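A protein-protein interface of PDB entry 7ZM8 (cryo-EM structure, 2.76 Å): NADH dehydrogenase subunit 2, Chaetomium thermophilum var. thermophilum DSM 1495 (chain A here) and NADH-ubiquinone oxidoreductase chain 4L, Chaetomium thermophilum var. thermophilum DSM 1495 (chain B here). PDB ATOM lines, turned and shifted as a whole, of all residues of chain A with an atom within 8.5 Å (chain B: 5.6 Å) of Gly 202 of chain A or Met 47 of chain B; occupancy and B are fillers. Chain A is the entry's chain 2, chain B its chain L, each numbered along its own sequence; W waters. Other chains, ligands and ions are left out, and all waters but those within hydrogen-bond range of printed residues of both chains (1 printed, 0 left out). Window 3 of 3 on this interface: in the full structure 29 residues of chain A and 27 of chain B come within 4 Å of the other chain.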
ATOM      1  N   LEU A 145     -20.618 -14.063   1.265  1.00  0.00           N
ATOM      2  CA  LEU A 145     -20.109 -15.033   2.259  1.00  0.00           C
ATOM      3  C   LEU A 145     -19.190 -14.269   3.191  1.00  0.00           C
ATOM      4  O   LEU A 145     -19.259 -14.516   4.394  1.00  0.00           O
ATOM      5  CB  LEU A 145     -19.340 -16.120   1.501  1.00  0.00           C
ATOM      6  CG  LEU A 145     -20.209 -17.126   0.749  1.00  0.00           C
ATOM      7  CD1 LEU A 145     -19.351 -18.113  -0.022  1.00  0.00           C
ATOM      8  CD2 LEU A 145     -21.143 -17.855   1.697  1.00  0.00           C
ATOM      9  N   SER A 195     -16.119 -21.416   3.230  1.00  0.00           N
ATOM     10  CA  SER A 195     -14.948 -21.771   2.437  1.00  0.00           C
ATOM     11  C   SER A 195     -15.271 -22.870   1.436  1.00  0.00           C
ATOM     12  O   SER A 195     -14.868 -22.796   0.272  1.00  0.00           O
ATOM     13  CB  SER A 195     -13.812 -22.211   3.355  1.00  0.00           C
ATOM     14  OG  SER A 195     -13.917 -23.590   3.657  1.00  0.00           O
ATOM     15  N   LEU A 196     -15.995 -23.899   1.869  1.00  0.00           N
ATOM     16  CA  LEU A 196     -16.358 -24.983   0.968  1.00  0.00           C
ATOM     17  C   LEU A 196     -17.360 -24.546  -0.084  1.00  0.00           C
ATOM     18  O   LEU A 196     -17.480 -25.207  -1.119  1.00  0.00           O
ATOM     19  CB  LEU A 196     -16.921 -26.158   1.760  1.00  0.00           C
ATOM     20  CG  LEU A 196     -15.883 -27.079   2.380  1.00  0.00           C
ATOM     21  CD1 LEU A 196     -16.567 -28.006   3.337  1.00  0.00           C
ATOM     22  CD2 LEU A 196     -15.166 -27.850   1.309  1.00  0.00           C
ATOM     23  N   LEU A 197     -18.088 -23.460   0.159  1.00  0.00           N
ATOM     24  CA  LEU A 197     -18.973 -22.928  -0.866  1.00  0.00           C
ATOM     25  C   LEU A 197     -18.183 -22.258  -1.977  1.00  0.00           C
ATOM     26  O   LEU A 197     -18.453 -22.486  -3.159  1.00  0.00           O
ATOM     27  CB  LEU A 197     -19.958 -21.946  -0.244  1.00  0.00           C
ATOM     28  CG  LEU A 197     -21.203 -22.575   0.367  1.00  0.00           C
ATOM     29  CD1 LEU A 197     -21.810 -21.654   1.402  1.00  0.00           C
ATOM     30  CD2 LEU A 197     -22.199 -22.914  -0.708  1.00  0.00           C
ATOM     31  N   TYR A 198     -17.191 -21.448  -1.614  1.00  0.00           N
ATOM     32  CA  TYR A 198     -16.453 -20.672  -2.602  1.00  0.00           C
ATOM     33  C   TYR A 198     -15.565 -21.561  -3.468  1.00  0.00           C
ATOM     34  O   TYR A 198     -15.445 -21.336  -4.674  1.00  0.00           O
ATOM     35  CB  TYR A 198     -15.641 -19.587  -1.887  1.00  0.00           C
ATOM     36  CG  TYR A 198     -14.596 -18.902  -2.728  1.00  0.00           C
ATOM     37  CD1 TYR A 198     -14.943 -17.921  -3.641  1.00  0.00           C
ATOM     38  CD2 TYR A 198     -13.256 -19.231  -2.598  1.00  0.00           C
ATOM     39  CE1 TYR A 198     -13.997 -17.299  -4.407  1.00  0.00           C
ATOM     40  CE2 TYR A 198     -12.297 -18.615  -3.367  1.00  0.00           C
ATOM     41  CZ  TYR A 198     -12.672 -17.648  -4.267  1.00  0.00           C
ATOM     42  OH  TYR A 198     -11.716 -17.029  -5.032  1.00  0.00           O
ATOM     43  N   VAL A 199     -15.025 -22.635  -2.902  1.00  0.00           N
ATOM     44  CA  VAL A 199     -14.080 -23.530  -3.624  1.00  0.00           C
ATOM     45  C   VAL A 199     -14.804 -24.372  -4.674  1.00  0.00           C
ATOM     46  O   VAL A 199     -14.149 -24.839  -5.599  1.00  0.00           O
ATOM     47  CB  VAL A 199     -13.259 -24.399  -2.651  1.00  0.00           C
ATOM     48  CG1 VAL A 199     -12.469 -23.551  -1.670  1.00  0.00           C
ATOM     49  CG2 VAL A 199     -14.100 -25.430  -1.921  1.00  0.00           C
ATOM     50  N   ASN A 200     -16.113 -24.551  -4.530  1.00  0.00           N
ATOM     51  CA  ASN A 200     -16.870 -25.420  -5.456  1.00  0.00           C
ATOM     52  C   ASN A 200     -17.695 -24.590  -6.416  1.00  0.00           C
ATOM     53  O   ASN A 200     -18.204 -25.161  -7.369  1.00  0.00           O
ATOM     54  CB  ASN A 200     -17.707 -26.431  -4.683  1.00  0.00           C
ATOM     55  CG  ASN A 200     -16.889 -27.548  -4.074  1.00  0.00           C
ATOM     56  OD1 ASN A 200     -16.253 -28.317  -4.785  1.00  0.00           O
ATOM     57  ND2 ASN A 200     -16.907 -27.653  -2.758  1.00  0.00           N
ATOM     58  N   SER A 201     -17.784 -23.290  -6.190  1.00  0.00           N
ATOM     59  CA  SER A 201     -18.655 -22.411  -6.996  1.00  0.00           C
ATOM     60  C   SER A 201     -17.880 -21.256  -7.617  1.00  0.00           C
ATOM     61  O   SER A 201     -18.394 -20.675  -8.561  1.00  0.00           O
ATOM     62  CB  SER A 201     -19.704 -21.881  -6.105  1.00  0.00           C
ATOM     63  OG  SER A 201     -19.151 -20.991  -5.159  1.00  0.00           O
ATOM     64  N   GLY A 202     -16.734 -20.882  -7.076  1.00  0.00           N
ATOM     65  CA  GLY A 202     -15.980 -19.705  -7.544  1.00  0.00           C
ATOM     66  C   GLY A 202     -16.604 -18.387  -7.157  1.00  0.00           C
ATOM     67  O   GLY A 202     -16.092 -17.368  -7.589  1.00  0.00           O
ATOM     68  N   THR A 203     -17.649 -18.395  -6.342  1.00  0.00           N
ATOM     69  CA  THR A 203     -18.396 -17.160  -6.044  1.00  0.00           C
ATOM     70  C   THR A 203     -18.500 -16.945  -4.547  1.00  0.00           C
ATOM     71  O   THR A 203     -18.434 -17.932  -3.818  1.00  0.00           O
ATOM     72  CB  THR A 203     -19.814 -17.203  -6.639  1.00  0.00           C
ATOM     73  OG1 THR A 203     -20.403 -15.912  -6.479  1.00  0.00           O
ATOM     74  CG2 THR A 203     -20.724 -18.257  -6.053  1.00  0.00           C
ATOM     75  N   THR A 204     -18.658 -15.697  -4.122  1.00  0.00           N
ATOM     76  CA  THR A 204     -18.849 -15.378  -2.692  1.00  0.00           C
ATOM     77  C   THR A 204     -20.248 -14.779  -2.542  1.00  0.00           C
ATOM     78  O   THR A 204     -20.716 -14.682  -1.409  1.00  0.00           O
ATOM     79  CB  THR A 204     -17.736 -14.442  -2.218  1.00  0.00           C
ATOM     80  OG1 THR A 204     -17.572 -13.432  -3.212  1.00  0.00           O
ATOM     81  CG2 THR A 204     -16.414 -15.140  -1.992  1.00  0.00           C
ATOM     82  N   SER A 205     -20.885 -14.419  -3.661  1.00  0.00           N
ATOM     83  CA  SER A 205     -22.235 -13.802  -3.677  1.00  0.00           C
ATOM     84  C   SER A 205     -23.338 -14.831  -3.437  1.00  0.00           C
ATOM     85  O   SER A 205     -23.309 -15.882  -4.085  1.00  0.00           O
ATOM     86  CB  SER A 205     -22.442 -13.156  -5.000  1.00  0.00           C
ATOM     87  OG  SER A 205     -22.629 -14.122  -6.018  1.00  0.00           O
ATOM     88  N   LEU A 209     -24.926 -18.165  -5.973  1.00  0.00           N
ATOM     89  CA  LEU A 209     -25.162 -19.498  -5.377  1.00  0.00           C
ATOM     90  C   LEU A 209     -26.638 -19.858  -5.500  1.00  0.00           C
ATOM     91  O   LEU A 209     -26.924 -21.044  -5.698  1.00  0.00           O
ATOM     92  CB  LEU A 209     -24.764 -19.404  -3.906  1.00  0.00           C
ATOM     93  CG  LEU A 209     -23.269 -19.510  -3.619  1.00  0.00           C
ATOM     94  CD1 LEU A 209     -22.965 -19.117  -2.183  1.00  0.00           C
ATOM     95  CD2 LEU A 209     -22.763 -20.915  -3.907  1.00  0.00           C
ATOM     96  N   LEU A 212     -27.139 -20.777  -9.153  1.00  0.00           N
ATOM     97  CA  LEU A 212     -26.509 -22.096  -9.417  1.00  0.00           C
ATOM     98  C   LEU A 212     -27.440 -23.179  -8.875  1.00  0.00           C
ATOM     99  O   LEU A 212     -27.638 -24.180  -9.572  1.00  0.00           O
ATOM    100  CB  LEU A 212     -25.127 -22.152  -8.758  1.00  0.00           C
ATOM    101  CG  LEU A 212     -24.027 -21.342  -9.442  1.00  0.00           C
ATOM    102  CD1 LEU A 212     -22.768 -21.307  -8.590  1.00  0.00           C
ATOM    103  CD2 LEU A 212     -23.720 -21.896 -10.823  1.00  0.00           C
ATOM    104  N   TYR A 239     -22.391 -30.181  -3.203  1.00  0.00           N
ATOM    105  CA  TYR A 239     -21.663 -29.305  -2.254  1.00  0.00           C
ATOM    106  C   TYR A 239     -22.584 -28.308  -1.567  1.00  0.00           C
ATOM    107  O   TYR A 239     -22.307 -28.012  -0.413  1.00  0.00           O
ATOM    108  CB  TYR A 239     -20.535 -28.556  -2.968  1.00  0.00           C
ATOM    109  CG  TYR A 239     -20.962 -27.441  -3.889  1.00  0.00           C
ATOM    110  CD1 TYR A 239     -21.335 -27.695  -5.197  1.00  0.00           C
ATOM    111  CD2 TYR A 239     -20.971 -26.124  -3.458  1.00  0.00           C
ATOM    112  CE1 TYR A 239     -21.722 -26.674  -6.046  1.00  0.00           C
ATOM    113  CE2 TYR A 239     -21.359 -25.091  -4.293  1.00  0.00           C
ATOM    114  CZ  TYR A 239     -21.734 -25.368  -5.594  1.00  0.00           C
ATOM    115  OH  TYR A 239     -22.115 -24.357  -6.423  1.00  0.00           O
ATOM    116  N   LEU B  42      -5.353 -21.924  -1.943  1.00  0.00           N
ATOM    117  CA  LEU B  42      -4.898 -22.882  -2.987  1.00  0.00           C
ATOM    118  C   LEU B  42      -5.983 -22.976  -4.053  1.00  0.00           C
ATOM    119  O   LEU B  42      -5.628 -23.082  -5.222  1.00  0.00           O
ATOM    120  CB  LEU B  42      -4.618 -24.255  -2.371  1.00  0.00           C
ATOM    121  CG  LEU B  42      -3.430 -24.363  -1.424  1.00  0.00           C
ATOM    122  CD1 LEU B  42      -3.036 -25.817  -1.240  1.00  0.00           C
ATOM    123  CD2 LEU B  42      -2.261 -23.566  -1.949  1.00  0.00           C
ATOM    124  N   SER B  43      -7.249 -22.917  -3.657  1.00  0.00           N
ATOM    125  CA  SER B  43      -8.307 -22.878  -4.653  1.00  0.00           C
ATOM    126  C   SER B  43      -8.344 -21.554  -5.393  1.00  0.00           C
ATOM    127  O   SER B  43      -8.922 -21.478  -6.479  1.00  0.00           O
ATOM    128  CB  SER B  43      -9.656 -23.145  -3.989  1.00  0.00           C
ATOM    129  OG  SER B  43      -9.612 -24.336  -3.226  1.00  0.00           O
ATOM    130  N   SER B  44      -7.832 -20.493  -4.800  1.00  0.00           N
ATOM    131  CA  SER B  44      -7.782 -19.154  -5.444  1.00  0.00           C
ATOM    132  C   SER B  44      -6.766 -19.168  -6.584  1.00  0.00           C
ATOM    133  O   SER B  44      -7.111 -18.693  -7.664  1.00  0.00           O
ATOM    134  CB  SER B  44      -7.504 -18.113  -4.423  1.00  0.00           C
ATOM    135  OG  SER B  44      -8.512 -18.138  -3.433  1.00  0.00           O
ATOM    136  N   LEU B  45      -5.570 -19.703  -6.344  1.00  0.00           N
ATOM    137  CA  LEU B  45      -4.545 -19.863  -7.404  1.00  0.00           C
ATOM    138  C   LEU B  45      -5.091 -20.770  -8.519  1.00  0.00           C
ATOM    139  O   LEU B  45      -4.709 -20.553  -9.673  1.00  0.00           O
ATOM    140  CB  LEU B  45      -3.293 -20.448  -6.745  1.00  0.00           C
ATOM    141  CG  LEU B  45      -2.022 -20.478  -7.586  1.00  0.00           C
ATOM    142  CD1 LEU B  45      -1.511 -19.069  -7.829  1.00  0.00           C
ATOM    143  CD2 LEU B  45      -0.959 -21.311  -6.891  1.00  0.00           C
ATOM    144  N   ASN B  46      -5.974 -21.712  -8.205  1.00  0.00           N
ATOM    145  CA  ASN B  46      -6.458 -22.671  -9.233  1.00  0.00           C
ATOM    146  C   ASN B  46      -7.533 -22.031 -10.101  1.00  0.00           C
ATOM    147  O   ASN B  46      -7.703 -22.517 -11.214  1.00  0.00           O
ATOM    148  CB  ASN B  46      -7.031 -23.943  -8.607  1.00  0.00           C
ATOM    149  CG  ASN B  46      -5.991 -24.802  -7.926  1.00  0.00           C
ATOM    150  OD1 ASN B  46      -4.795 -24.637  -8.148  1.00  0.00           O
ATOM    151  ND2 ASN B  46      -6.440 -25.723  -7.093  1.00  0.00           N
ATOM    152  N   MET B  47      -8.140 -20.925  -9.664  1.00  0.00           N
ATOM    153  CA  MET B  47      -9.247 -20.274 -10.413  1.00  0.00           C
ATOM    154  C   MET B  47      -8.868 -18.864 -10.854  1.00  0.00           C
ATOM    155  O   MET B  47      -9.755 -18.189 -11.383  1.00  0.00           O
ATOM    156  CB  MET B  47     -10.500 -20.218  -9.538  1.00  0.00           C
ATOM    157  CG  MET B  47     -10.974 -21.571  -9.046  1.00  0.00           C
ATOM    158  SD  MET B  47     -12.502 -21.492  -8.065  1.00  0.00           S
ATOM    159  CE  MET B  47     -12.101 -20.198  -6.894  1.00  0.00           C
ATOM    160  N   ASP B  48      -7.614 -18.452 -10.684  1.00  0.00           N
ATOM    161  CA  ASP B  48      -7.118 -17.095 -11.059  1.00  0.00           C
ATOM    162  C   ASP B  48      -7.977 -16.009 -10.423  1.00  0.00           C
ATOM    163  O   ASP B  48      -8.360 -15.081 -11.135  1.00  0.00           O
ATOM    164  CB  ASP B  48      -7.005 -16.897 -12.568  1.00  0.00           C
ATOM    165  CG  ASP B  48      -6.149 -15.706 -12.966  1.00  0.00           C
ATOM    166  OD1 ASP B  48      -4.982 -15.659 -12.536  1.00  0.00           O
ATOM    167  OD2 ASP B  48      -6.664 -14.827 -13.691  1.00  0.00           O
ATOM    168  N   ASP B  49      -8.265 -16.127  -9.137  1.00  0.00           N
ATOM    169  CA  ASP B  49      -9.187 -15.166  -8.485  1.00  0.00           C
ATOM    170  C   ASP B  49      -8.460 -14.478  -7.333  1.00  0.00           C
ATOM    171  O   ASP B  49      -8.050 -15.163  -6.396  1.00  0.00           O
ATOM    172  CB  ASP B  49     -10.474 -15.868  -8.057  1.00  0.00           C
ATOM    173  CG  ASP B  49     -11.703 -14.981  -8.132  1.00  0.00           C
ATOM    174  OD1 ASP B  49     -11.552 -13.814  -8.541  1.00  0.00           O
ATOM    175  OD2 ASP B  49     -12.800 -15.464  -7.781  1.00  0.00           O
HETATM  176  O   HOH W   1     -11.524 -24.270  -6.289  1.00  0.00           O
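O of Ser 44 of chain B lies within hydrogen-bond range of N of Asp 49 of chain B, 3.2 Å away.
Hydrophobic or aromatic side chains of chain B that line the printed part of chain A: Met 47. Of the 15 printed residues of chain A, 3 touch a printed residue of chain B. Among the printed residues, 6 pairs touch across the chains.
Gly 202 of chain A touches just these residues of chain B: Met 47 (3.9 Å) and Asp 49 (3.8 Å). Leu 209 of chain A touches none of the printed residues of chain B. Of the printed residues of chain A, Ser 43 of chain B touches Val 199. Of the printed residues of chain A, Ser 44 of chain B touches Tyr 198. Of chain A, only Tyr 198 and Gly 202 come within 4 Å of Met 47 of chain B. Of the printed residues of chain A, Asp 49 of chain B touches Tyr 198 and Gly 202. The nearest printed residue of chain B that does not touch Gly 202 of chain A is Ser 43 of chain B (7.4 Å).
OD2 of Asp 49 of chain B lies within hydrogen-bond range of OH of Tyr 198 of chain A, at 3.3 Å.
Water W1 lies within hydrogen-bond range of the backbone carbonyl oxygen (O) of Val 199 of chain A (2.8 Å) and the side-chain sulfur (SD) of Met 47 of chain B (3.4 Å).
Among the printed residues, pairs that only touch across the chains: Tyr 198 of chain A with Ser 44 of chain B (3.7 Å), Tyr 198 of chain A with Met 47 of chain B (3.7 Å), Val 199 of chain A with Ser 43 of chain B (3.3 Å), Gly 202 of chain A with Met 47 of chain B (3.9 Å) and Gly 202 of chain A with Asp 49 of chain B (3.8 Å).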
